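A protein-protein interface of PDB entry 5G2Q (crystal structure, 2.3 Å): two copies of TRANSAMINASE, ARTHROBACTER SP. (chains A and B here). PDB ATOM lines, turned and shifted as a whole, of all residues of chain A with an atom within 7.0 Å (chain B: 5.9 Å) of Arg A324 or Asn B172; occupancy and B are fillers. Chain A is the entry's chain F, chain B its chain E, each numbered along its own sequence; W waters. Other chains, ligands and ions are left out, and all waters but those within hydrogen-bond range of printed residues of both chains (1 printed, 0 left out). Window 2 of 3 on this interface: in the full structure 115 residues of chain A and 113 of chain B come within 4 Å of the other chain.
The backbone carbonyl oxygen (O) of His B410 lies within hydrogen-bond range of the guanidinium group (NH1) of Arg A324, at 2.8 Å. O of Met B412 sits at hydrogen-bond distance from NH1 of Arg A324, 3.2 Å away. The backbone carbonyl oxygen (O) of Trp A325 lies within hydrogen-bond range of the backbone NH (N) of Phe B25, 2.6 Å away. A ring nitrogen (ND1) of His B410 sits at hydrogen-bond distance from the side-chain carboxylate (OE2) of Glu A326 (2.6 Å). The side-chain carboxylate (OE2) of Glu B30 lies within salt-bridge range of the guanidinium group (NE) of Arg A324. The backbone NH (N) of Arg A324 sits at hydrogen-bond distance from the backbone carbonyl oxygen (O) of Val B169 (2.7 Å). NH2 of Arg A324 is in hydrogen-bond range of OD1 of Asn B172 (2.9 Å). The backbone carbonyl oxygen of Gly B167 sits at hydrogen-bond distance from the backbone NH of Glu A326, 3.0 Å away.
The side-chain carboxylate (OE2) of Glu B30 is in hydrogen-bond range of the backbone NH (N) of Thr B27, at 3.1 Å. O of Gly B411 sits close to N of Asn B172 (3.4 Å). The side-chain hydroxyl (OG1) of Thr B27 sits at hydrogen-bond distance from the side-chain carboxylate (OE1) of Glu B171 (2.6 Å). N of Ser B173 sits at hydrogen-bond distance from O of Gly B411, at 2.8 Å.
Thr B27 touches Asp A321 (CA to O, 3.4 Å). His A323 touches Leu B168 (ND1 to CD1, 3.7 Å). Val B169 touches His A323. Phe B25 touches Arg A324. Leu B168 touches Arg A324. Arg A324 touches Glu B171 (NH2 to CG, 3.3 Å). Gly B411 touches Arg A324 (O to NH1, 3.7 Å). O of Trp A325 touches C of Thr B24, 3.5 Å away. Trp A325 touches Leu B168. CA of Glu A326 touches CE1 of Phe B25, at 3.7 Å.
Met A320 touches none of the printed residues of chain B. Of chain B, only Phe B25 (3.5 Å), Thr B27 (3.9 Å), Glu B30 (2.7 Å), Gly B167 (3.7 Å), Leu B168 (3.5 Å), Val B169 (2.7 Å), Gly B170 (3.6 Å), Glu B171 (3.3 Å), Asn B172 (2.9 Å), His B410 (2.8 Å), Gly B411 (3.7 Å) and Met B412 (3.2 Å) come within 4 Å of Arg A324. Of the printed residues of chain B, Ser A327 touches Thr B24 (3.5 Å) and Phe B25 (3.9 Å). Of the printed residues of chain A, Leu B168 touches His A323 (3.7 Å), Arg A324 (3.5 Å) and Trp A325 (3.6 Å). Printed residues of chain A within 4 Å of Val B169: His A323, Arg A324 and Glu A326. Of the printed residues of chain A, Asn B172 touches Arg A324 (2.9 Å). The nearest printed residue of chain A that does not touch Asn B172 is Lys A322 (8.2 Å). The nearest printed residue of chain A that does not touch Glu B30 is His A323 (6.4 Å).
Of the 18 printed residues of chain B, 14 touch a printed residue of chain A. Of the 8 printed residues of chain A, 7 touch a printed residue of chain B. Among the printed residues, Asp or Glu carboxylates within 4 Å of a Lys or Arg side-chain nitrogen of the other chain: Arg A324 with Glu B30.
No position is printed for both chains. Of the 28 pairs that touch across the chains among the printed residues, none has its exchanged pair printed and touching as well.
Water W1 lies within hydrogen-bond range of OG1 of Thr B24 (2.6 Å) and O of Ser A327 (2.8 Å).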
ATOM      1  N   MET A 320      -1.136  15.239   7.961  1.00  0.00           N
ATOM      2  CA  MET A 320      -1.585  15.961   9.168  1.00  0.00           C
ATOM      3  C   MET A 320      -1.506  17.503   9.030  1.00  0.00           C
ATOM      4  O   MET A 320      -2.305  18.228   9.631  1.00  0.00           O
ATOM      5  CB  MET A 320      -0.935  15.424  10.430  1.00  0.00           C
ATOM      6  CG  MET A 320      -1.274  13.960  10.666  1.00  0.00           C
ATOM      7  SD  MET A 320      -2.871  13.652  11.476  1.00  0.00           S
ATOM      8  CE  MET A 320      -2.432  14.550  12.973  1.00  0.00           C
ATOM      9  N   ASP A 321      -0.593  17.987   8.182  1.00  0.00           N
ATOM     10  CA  ASP A 321      -0.368  19.429   8.007  1.00  0.00           C
ATOM     11  C   ASP A 321      -1.499  20.101   7.249  1.00  0.00           C
ATOM     12  O   ASP A 321      -1.708  21.288   7.396  1.00  0.00           O
ATOM     13  CB  ASP A 321       0.940  19.692   7.243  1.00  0.00           C
ATOM     14  CG  ASP A 321       2.169  19.750   8.145  1.00  0.00           C
ATOM     15  OD1 ASP A 321       2.053  19.607   9.397  1.00  0.00           O
ATOM     16  OD2 ASP A 321       3.258  19.955   7.564  1.00  0.00           O
ATOM     17  N   LYS A 322      -2.194  19.320   6.428  1.00  0.00           N
ATOM     18  CA  LYS A 322      -3.300  19.761   5.563  1.00  0.00           C
ATOM     19  C   LYS A 322      -4.627  20.004   6.310  1.00  0.00           C
ATOM     20  O   LYS A 322      -5.631  20.368   5.709  1.00  0.00           O
ATOM     21  CB  LYS A 322      -3.543  18.666   4.520  1.00  0.00           C
ATOM     22  CG  LYS A 322      -2.622  18.708   3.311  1.00  0.00           C
ATOM     23  CD  LYS A 322      -2.791  17.478   2.441  1.00  0.00           C
ATOM     24  CE  LYS A 322      -4.254  17.112   2.193  1.00  0.00           C
ATOM     25  NZ  LYS A 322      -4.372  15.620   2.325  1.00  0.00           N
ATOM     26  N   HIS A 323      -4.631  19.768   7.617  1.00  0.00           N
ATOM     27  CA  HIS A 323      -5.863  19.666   8.391  1.00  0.00           C
ATOM     28  C   HIS A 323      -5.667  20.369   9.708  1.00  0.00           C
ATOM     29  O   HIS A 323      -4.561  20.516  10.172  1.00  0.00           O
ATOM     30  CB  HIS A 323      -6.203  18.189   8.703  1.00  0.00           C
ATOM     31  CG  HIS A 323      -6.574  17.369   7.510  1.00  0.00           C
ATOM     32  ND1 HIS A 323      -5.934  16.192   7.193  1.00  0.00           N
ATOM     33  CD2 HIS A 323      -7.528  17.546   6.566  1.00  0.00           C
ATOM     34  CE1 HIS A 323      -6.481  15.672   6.111  1.00  0.00           C
ATOM     35  NE2 HIS A 323      -7.446  16.478   5.706  1.00  0.00           N
ATOM     36  N   ARG A 324      -6.766  20.811  10.296  1.00  0.00           N
ATOM     37  CA  ARG A 324      -6.781  21.311  11.647  1.00  0.00           C
ATOM     38  C   ARG A 324      -7.009  20.131  12.588  1.00  0.00           C
ATOM     39  O   ARG A 324      -8.017  19.434  12.493  1.00  0.00           O
ATOM     40  CB  ARG A 324      -7.894  22.323  11.778  1.00  0.00           C
ATOM     41  CG  ARG A 324      -7.749  23.466  10.800  1.00  0.00           C
ATOM     42  CD  ARG A 324      -8.692  24.594  11.146  1.00  0.00           C
ATOM     43  NE  ARG A 324      -8.405  25.766  10.323  1.00  0.00           N
ATOM     44  CZ  ARG A 324      -9.318  26.608   9.842  1.00  0.00           C
ATOM     45  NH1 ARG A 324     -10.608  26.427  10.090  1.00  0.00           N
ATOM     46  NH2 ARG A 324      -8.935  27.641   9.107  1.00  0.00           N
ATOM     47  N   TRP A 325      -6.061  19.913  13.487  1.00  0.00           N
ATOM     48  CA  TRP A 325      -6.099  18.781  14.381  1.00  0.00           C
ATOM     49  C   TRP A 325      -6.661  19.258  15.711  1.00  0.00           C
ATOM     50  O   TRP A 325      -6.117  20.178  16.334  1.00  0.00           O
ATOM     51  CB  TRP A 325      -4.695  18.184  14.527  1.00  0.00           C
ATOM     52  CG  TRP A 325      -4.639  16.864  15.177  1.00  0.00           C
ATOM     53  CD1 TRP A 325      -5.684  16.005  15.388  1.00  0.00           C
ATOM     54  CD2 TRP A 325      -3.473  16.197  15.660  1.00  0.00           C
ATOM     55  NE1 TRP A 325      -5.243  14.856  16.001  1.00  0.00           N
ATOM     56  CE2 TRP A 325      -3.888  14.944  16.177  1.00  0.00           C
ATOM     57  CE3 TRP A 325      -2.113  16.540  15.728  1.00  0.00           C
ATOM     58  CZ2 TRP A 325      -3.009  14.043  16.737  1.00  0.00           C
ATOM     59  CZ3 TRP A 325      -1.226  15.631  16.299  1.00  0.00           C
ATOM     60  CH2 TRP A 325      -1.686  14.392  16.786  1.00  0.00           C
ATOM     61  N   GLU A 326      -7.763  18.635  16.138  1.00  0.00           N
ATOM     62  CA  GLU A 326      -8.496  19.103  17.329  1.00  0.00           C
ATOM     63  C   GLU A 326      -8.080  18.404  18.628  1.00  0.00           C
ATOM     64  O   GLU A 326      -8.926  17.866  19.363  1.00  0.00           O
ATOM     65  CB  GLU A 326      -9.997  19.019  17.095  1.00  0.00           C
ATOM     66  CG  GLU A 326     -10.431  19.961  15.981  1.00  0.00           C
ATOM     67  CD  GLU A 326     -11.888  19.800  15.557  1.00  0.00           C
ATOM     68  OE1 GLU A 326     -12.318  18.666  15.315  1.00  0.00           O
ATOM     69  OE2 GLU A 326     -12.596  20.829  15.438  1.00  0.00           O
ATOM     70  N   SER A 327      -6.780  18.456  18.909  1.00  0.00           N
ATOM     71  CA  SER A 327      -6.203  17.705  19.984  1.00  0.00           C
ATOM     72  C   SER A 327      -5.397  18.588  20.906  1.00  0.00           C
ATOM     73  O   SER A 327      -4.471  19.284  20.472  1.00  0.00           O
ATOM     74  CB  SER A 327      -5.290  16.637  19.391  1.00  0.00           C
ATOM     75  OG  SER A 327      -5.107  15.579  20.311  1.00  0.00           O
ATOM     76  N   THR B  24      -1.327  21.742  15.703  1.00  0.00           N
ATOM     77  CA  THR B  24      -2.666  21.475  16.241  1.00  0.00           C
ATOM     78  C   THR B  24      -3.605  22.666  16.070  1.00  0.00           C
ATOM     79  O   THR B  24      -3.216  23.800  16.287  1.00  0.00           O
ATOM     80  CB  THR B  24      -2.696  21.001  17.705  1.00  0.00           C
ATOM     81  OG1 THR B  24      -1.936  21.875  18.537  1.00  0.00           O
ATOM     82  CG2 THR B  24      -2.154  19.601  17.832  1.00  0.00           C
ATOM     83  N   PHE B  25      -4.841  22.405  15.675  1.00  0.00           N
ATOM     84  CA  PHE B  25      -5.834  23.481  15.449  1.00  0.00           C
ATOM     85  C   PHE B  25      -5.603  24.368  14.234  1.00  0.00           C
ATOM     86  O   PHE B  25      -6.521  25.024  13.819  1.00  0.00           O
ATOM     87  CB  PHE B  25      -6.027  24.377  16.694  1.00  0.00           C
ATOM     88  CG  PHE B  25      -6.545  23.635  17.877  1.00  0.00           C
ATOM     89  CD1 PHE B  25      -7.839  23.105  17.861  1.00  0.00           C
ATOM     90  CD2 PHE B  25      -5.736  23.437  18.998  1.00  0.00           C
ATOM     91  CE1 PHE B  25      -8.326  22.402  18.945  1.00  0.00           C
ATOM     92  CE2 PHE B  25      -6.217  22.723  20.090  1.00  0.00           C
ATOM     93  CZ  PHE B  25      -7.516  22.196  20.056  1.00  0.00           C
ATOM     94  N   SER B  26      -4.375  24.408  13.715  1.00  0.00           N
ATOM     95  CA  SER B  26      -4.018  25.197  12.536  1.00  0.00           C
ATOM     96  C   SER B  26      -3.365  24.323  11.470  1.00  0.00           C
ATOM     97  O   SER B  26      -2.487  23.504  11.782  1.00  0.00           O
ATOM     98  CB  SER B  26      -3.035  26.312  12.902  1.00  0.00           C
ATOM     99  OG  SER B  26      -3.442  27.038  14.059  1.00  0.00           O
ATOM    100  N   THR B  27      -3.792  24.487  10.218  1.00  0.00           N
ATOM    101  CA  THR B  27      -3.087  23.869   9.108  1.00  0.00           C
ATOM    102  C   THR B  27      -1.678  24.481   8.958  1.00  0.00           C
ATOM    103  O   THR B  27      -1.449  25.650   9.322  1.00  0.00           O
ATOM    104  CB  THR B  27      -3.845  24.062   7.800  1.00  0.00           C
ATOM    105  OG1 THR B  27      -4.005  25.462   7.581  1.00  0.00           O
ATOM    106  CG2 THR B  27      -5.220  23.395   7.848  1.00  0.00           C
ATOM    107  N   GLU B  30      -1.798  27.937   7.144  1.00  0.00           N
ATOM    108  CA  GLU B  30      -2.290  29.144   7.810  1.00  0.00           C
ATOM    109  C   GLU B  30      -1.485  29.520   9.046  1.00  0.00           C
ATOM    110  O   GLU B  30      -1.584  30.623   9.549  1.00  0.00           O
ATOM    111  CB  GLU B  30      -3.767  28.984   8.186  1.00  0.00           C
ATOM    112  CG  GLU B  30      -4.034  27.919   9.248  1.00  0.00           C
ATOM    113  CD  GLU B  30      -5.496  27.821   9.653  1.00  0.00           C
ATOM    114  OE1 GLU B  30      -6.265  28.780   9.447  1.00  0.00           O
ATOM    115  OE2 GLU B  30      -5.881  26.773  10.181  1.00  0.00           O
ATOM    116  N   GLY B 167      -9.919  14.762  16.343  1.00  0.00           N
ATOM    117  CA  GLY B 167     -10.241  14.469  14.952  1.00  0.00           C
ATOM    118  C   GLY B 167      -9.629  15.506  14.040  1.00  0.00           C
ATOM    119  O   GLY B 167      -8.915  16.401  14.494  1.00  0.00           O
ATOM    120  N   LEU B 168      -9.914  15.393  12.748  1.00  0.00           N
ATOM    121  CA  LEU B 168      -9.416  16.344  11.762  1.00  0.00           C
ATOM    122  C   LEU B 168     -10.540  17.105  11.069  1.00  0.00           C
ATOM    123  O   LEU B 168     -11.485  16.503  10.575  1.00  0.00           O
ATOM    124  CB  LEU B 168      -8.572  15.645  10.707  1.00  0.00           C
ATOM    125  CG  LEU B 168      -7.362  14.836  11.225  1.00  0.00           C
ATOM    126  CD1 LEU B 168      -6.770  14.079  10.057  1.00  0.00           C
ATOM    127  CD2 LEU B 168      -6.320  15.764  11.869  1.00  0.00           C
ATOM    128  N   VAL B 169     -10.424  18.426  11.010  1.00  0.00           N
ATOM    129  CA  VAL B 169     -11.237  19.191  10.075  1.00  0.00           C
ATOM    130  C   VAL B 169     -10.359  19.918   9.054  1.00  0.00           C
ATOM    131  O   VAL B 169      -9.117  19.968   9.177  1.00  0.00           O
ATOM    132  CB  VAL B 169     -12.159  20.200  10.786  1.00  0.00           C
ATOM    133  CG1 VAL B 169     -13.302  19.480  11.480  1.00  0.00           C
ATOM    134  CG2 VAL B 169     -11.353  21.072  11.763  1.00  0.00           C
ATOM    135  N   GLY B 170     -11.014  20.463   8.041  1.00  0.00           N
ATOM    136  CA  GLY B 170     -10.336  21.219   7.005  1.00  0.00           C
ATOM    137  C   GLY B 170     -10.196  22.703   7.336  1.00  0.00           C
ATOM    138  O   GLY B 170     -10.600  23.188   8.404  1.00  0.00           O
ATOM    139  N   GLU B 171      -9.601  23.420   6.406  1.00  0.00           N
ATOM    140  CA  GLU B 171      -9.310  24.790   6.638  1.00  0.00           C
ATOM    141  C   GLU B 171     -10.351  25.651   5.893  1.00  0.00           C
ATOM    142  O   GLU B 171     -10.347  25.662   4.665  1.00  0.00           O
ATOM    143  CB  GLU B 171      -7.872  25.076   6.199  1.00  0.00           C
ATOM    144  CG  GLU B 171      -7.439  26.539   6.337  1.00  0.00           C
ATOM    145  CD  GLU B 171      -6.384  26.880   5.315  1.00  0.00           C
ATOM    146  OE1 GLU B 171      -5.219  26.436   5.482  1.00  0.00           O
ATOM    147  OE2 GLU B 171      -6.748  27.534   4.321  1.00  0.00           O
ATOM    148  N   ASN B 172     -11.198  26.344   6.674  1.00  0.00           N
ATOM    149  CA  ASN B 172     -12.407  27.059   6.226  1.00  0.00           C
ATOM    150  C   ASN B 172     -13.262  26.281   5.203  1.00  0.00           C
ATOM    151  O   ASN B 172     -13.413  26.660   4.039  1.00  0.00           O
ATOM    152  CB  ASN B 172     -12.093  28.488   5.743  1.00  0.00           C
ATOM    153  CG  ASN B 172     -11.003  29.171   6.564  1.00  0.00           C
ATOM    154  OD1 ASN B 172     -11.001  29.142   7.796  1.00  0.00           O
ATOM    155  ND2 ASN B 172     -10.083  29.829   5.868  1.00  0.00           N
ATOM    156  N   SER B 173     -13.851  25.191   5.664  1.00  0.00           N
ATOM    157  CA  SER B 173     -14.404  24.211   4.744  1.00  0.00           C
ATOM    158  C   SER B 173     -15.012  23.081   5.509  1.00  0.00           C
ATOM    159  O   SER B 173     -14.538  22.708   6.569  1.00  0.00           O
ATOM    160  CB  SER B 173     -13.292  23.640   3.866  1.00  0.00           C
ATOM    161  OG  SER B 173     -13.780  22.647   3.004  1.00  0.00           O
ATOM    162  N   GLU B 174     -16.060  22.524   4.932  1.00  0.00           N
ATOM    163  CA  GLU B 174     -16.810  21.443   5.544  1.00  0.00           C
ATOM    164  C   GLU B 174     -16.404  20.102   4.959  1.00  0.00           C
ATOM    165  O   GLU B 174     -16.801  19.067   5.468  1.00  0.00           O
ATOM    166  CB  GLU B 174     -18.312  21.693   5.330  1.00  0.00           C
ATOM    167  CG  GLU B 174     -18.832  22.936   6.041  1.00  0.00           C
ATOM    168  CD  GLU B 174     -18.432  22.970   7.516  1.00  0.00           C
ATOM    169  OE1 GLU B 174     -18.649  21.955   8.221  1.00  0.00           O
ATOM    170  OE2 GLU B 174     -17.891  24.007   7.980  1.00  0.00           O
ATOM    171  N   HIS B 410     -13.932  22.934  14.365  1.00  0.00           N
ATOM    172  CA  HIS B 410     -13.010  23.977  13.931  1.00  0.00           C
ATOM    173  C   HIS B 410     -12.837  24.086  12.417  1.00  0.00           C
ATOM    174  O   HIS B 410     -11.908  24.728  11.950  1.00  0.00           O
ATOM    175  CB  HIS B 410     -11.649  23.776  14.611  1.00  0.00           C
ATOM    176  CG  HIS B 410     -11.691  23.934  16.097  1.00  0.00           C
ATOM    177  ND1 HIS B 410     -11.933  22.881  16.951  1.00  0.00           N
ATOM    178  CD2 HIS B 410     -11.550  25.033  16.883  1.00  0.00           C
ATOM    179  CE1 HIS B 410     -11.930  23.313  18.199  1.00  0.00           C
ATOM    180  NE2 HIS B 410     -11.683  24.616  18.188  1.00  0.00           N
ATOM    181  N   GLY B 411     -13.733  23.490  11.635  1.00  0.00           N
ATOM    182  CA  GLY B 411     -13.613  23.586  10.180  1.00  0.00           C
ATOM    183  C   GLY B 411     -14.089  24.926   9.656  1.00  0.00           C
ATOM    184  O   GLY B 411     -13.811  25.312   8.508  1.00  0.00           O
ATOM    185  N   MET B 412     -14.811  25.646  10.498  1.00  0.00           N
ATOM    186  CA  MET B 412     -15.349  26.922  10.058  1.00  0.00           C
ATOM    187  C   MET B 412     -14.316  28.036  10.095  1.00  0.00           C
ATOM    188  O   MET B 412     -13.315  27.990  10.830  1.00  0.00           O
ATOM    189  CB  MET B 412     -16.625  27.302  10.814  1.00  0.00           C
ATOM    190  CG  MET B 412     -16.516  27.376  12.331  1.00  0.00           C
ATOM    191  SD  MET B 412     -18.130  27.633  13.131  1.00  0.00           S
ATOM    192  CE  MET B 412     -18.831  28.971  12.147  1.00  0.00           C
ATOM    193  N   ASN B 413     -14.567  29.022   9.255  1.00  0.00           N
ATOM    194  CA  ASN B 413     -13.768  30.243   9.202  1.00  0.00           C
ATOM    195  C   ASN B 413     -13.788  31.010  10.523  1.00  0.00           C
ATOM    196  O   ASN B 413     -14.856  31.467  10.939  1.00  0.00           O
ATOM    197  CB  ASN B 413     -14.249  31.140   8.062  1.00  0.00           C
ATOM    198  CG  ASN B 413     -13.159  32.039   7.559  1.00  0.00           C
ATOM    199  OD1 ASN B 413     -12.421  32.633   8.356  1.00  0.00           O
ATOM    200  ND2 ASN B 413     -13.041  32.153   6.237  1.00  0.00           N
ATOM    201  N   PRO B 414     -12.606  31.133  11.186  1.00  0.00           N
ATOM    202  CA  PRO B 414     -12.517  31.819  12.469  1.00  0.00           C
ATOM    203  C   PRO B 414     -13.056  33.270  12.418  1.00  0.00           C
ATOM    204  O   PRO B 414     -13.566  33.743  13.438  1.00  0.00           O
ATOM    205  CB  PRO B 414     -11.017  31.812  12.766  1.00  0.00           C
ATOM    206  CG  PRO B 414     -10.372  31.709  11.429  1.00  0.00           C
ATOM    207  CD  PRO B 414     -11.267  30.779  10.677  1.00  0.00           C
HETATM  208  O   HOH W   1      -2.818  21.453  21.000  1.00  0.00           O
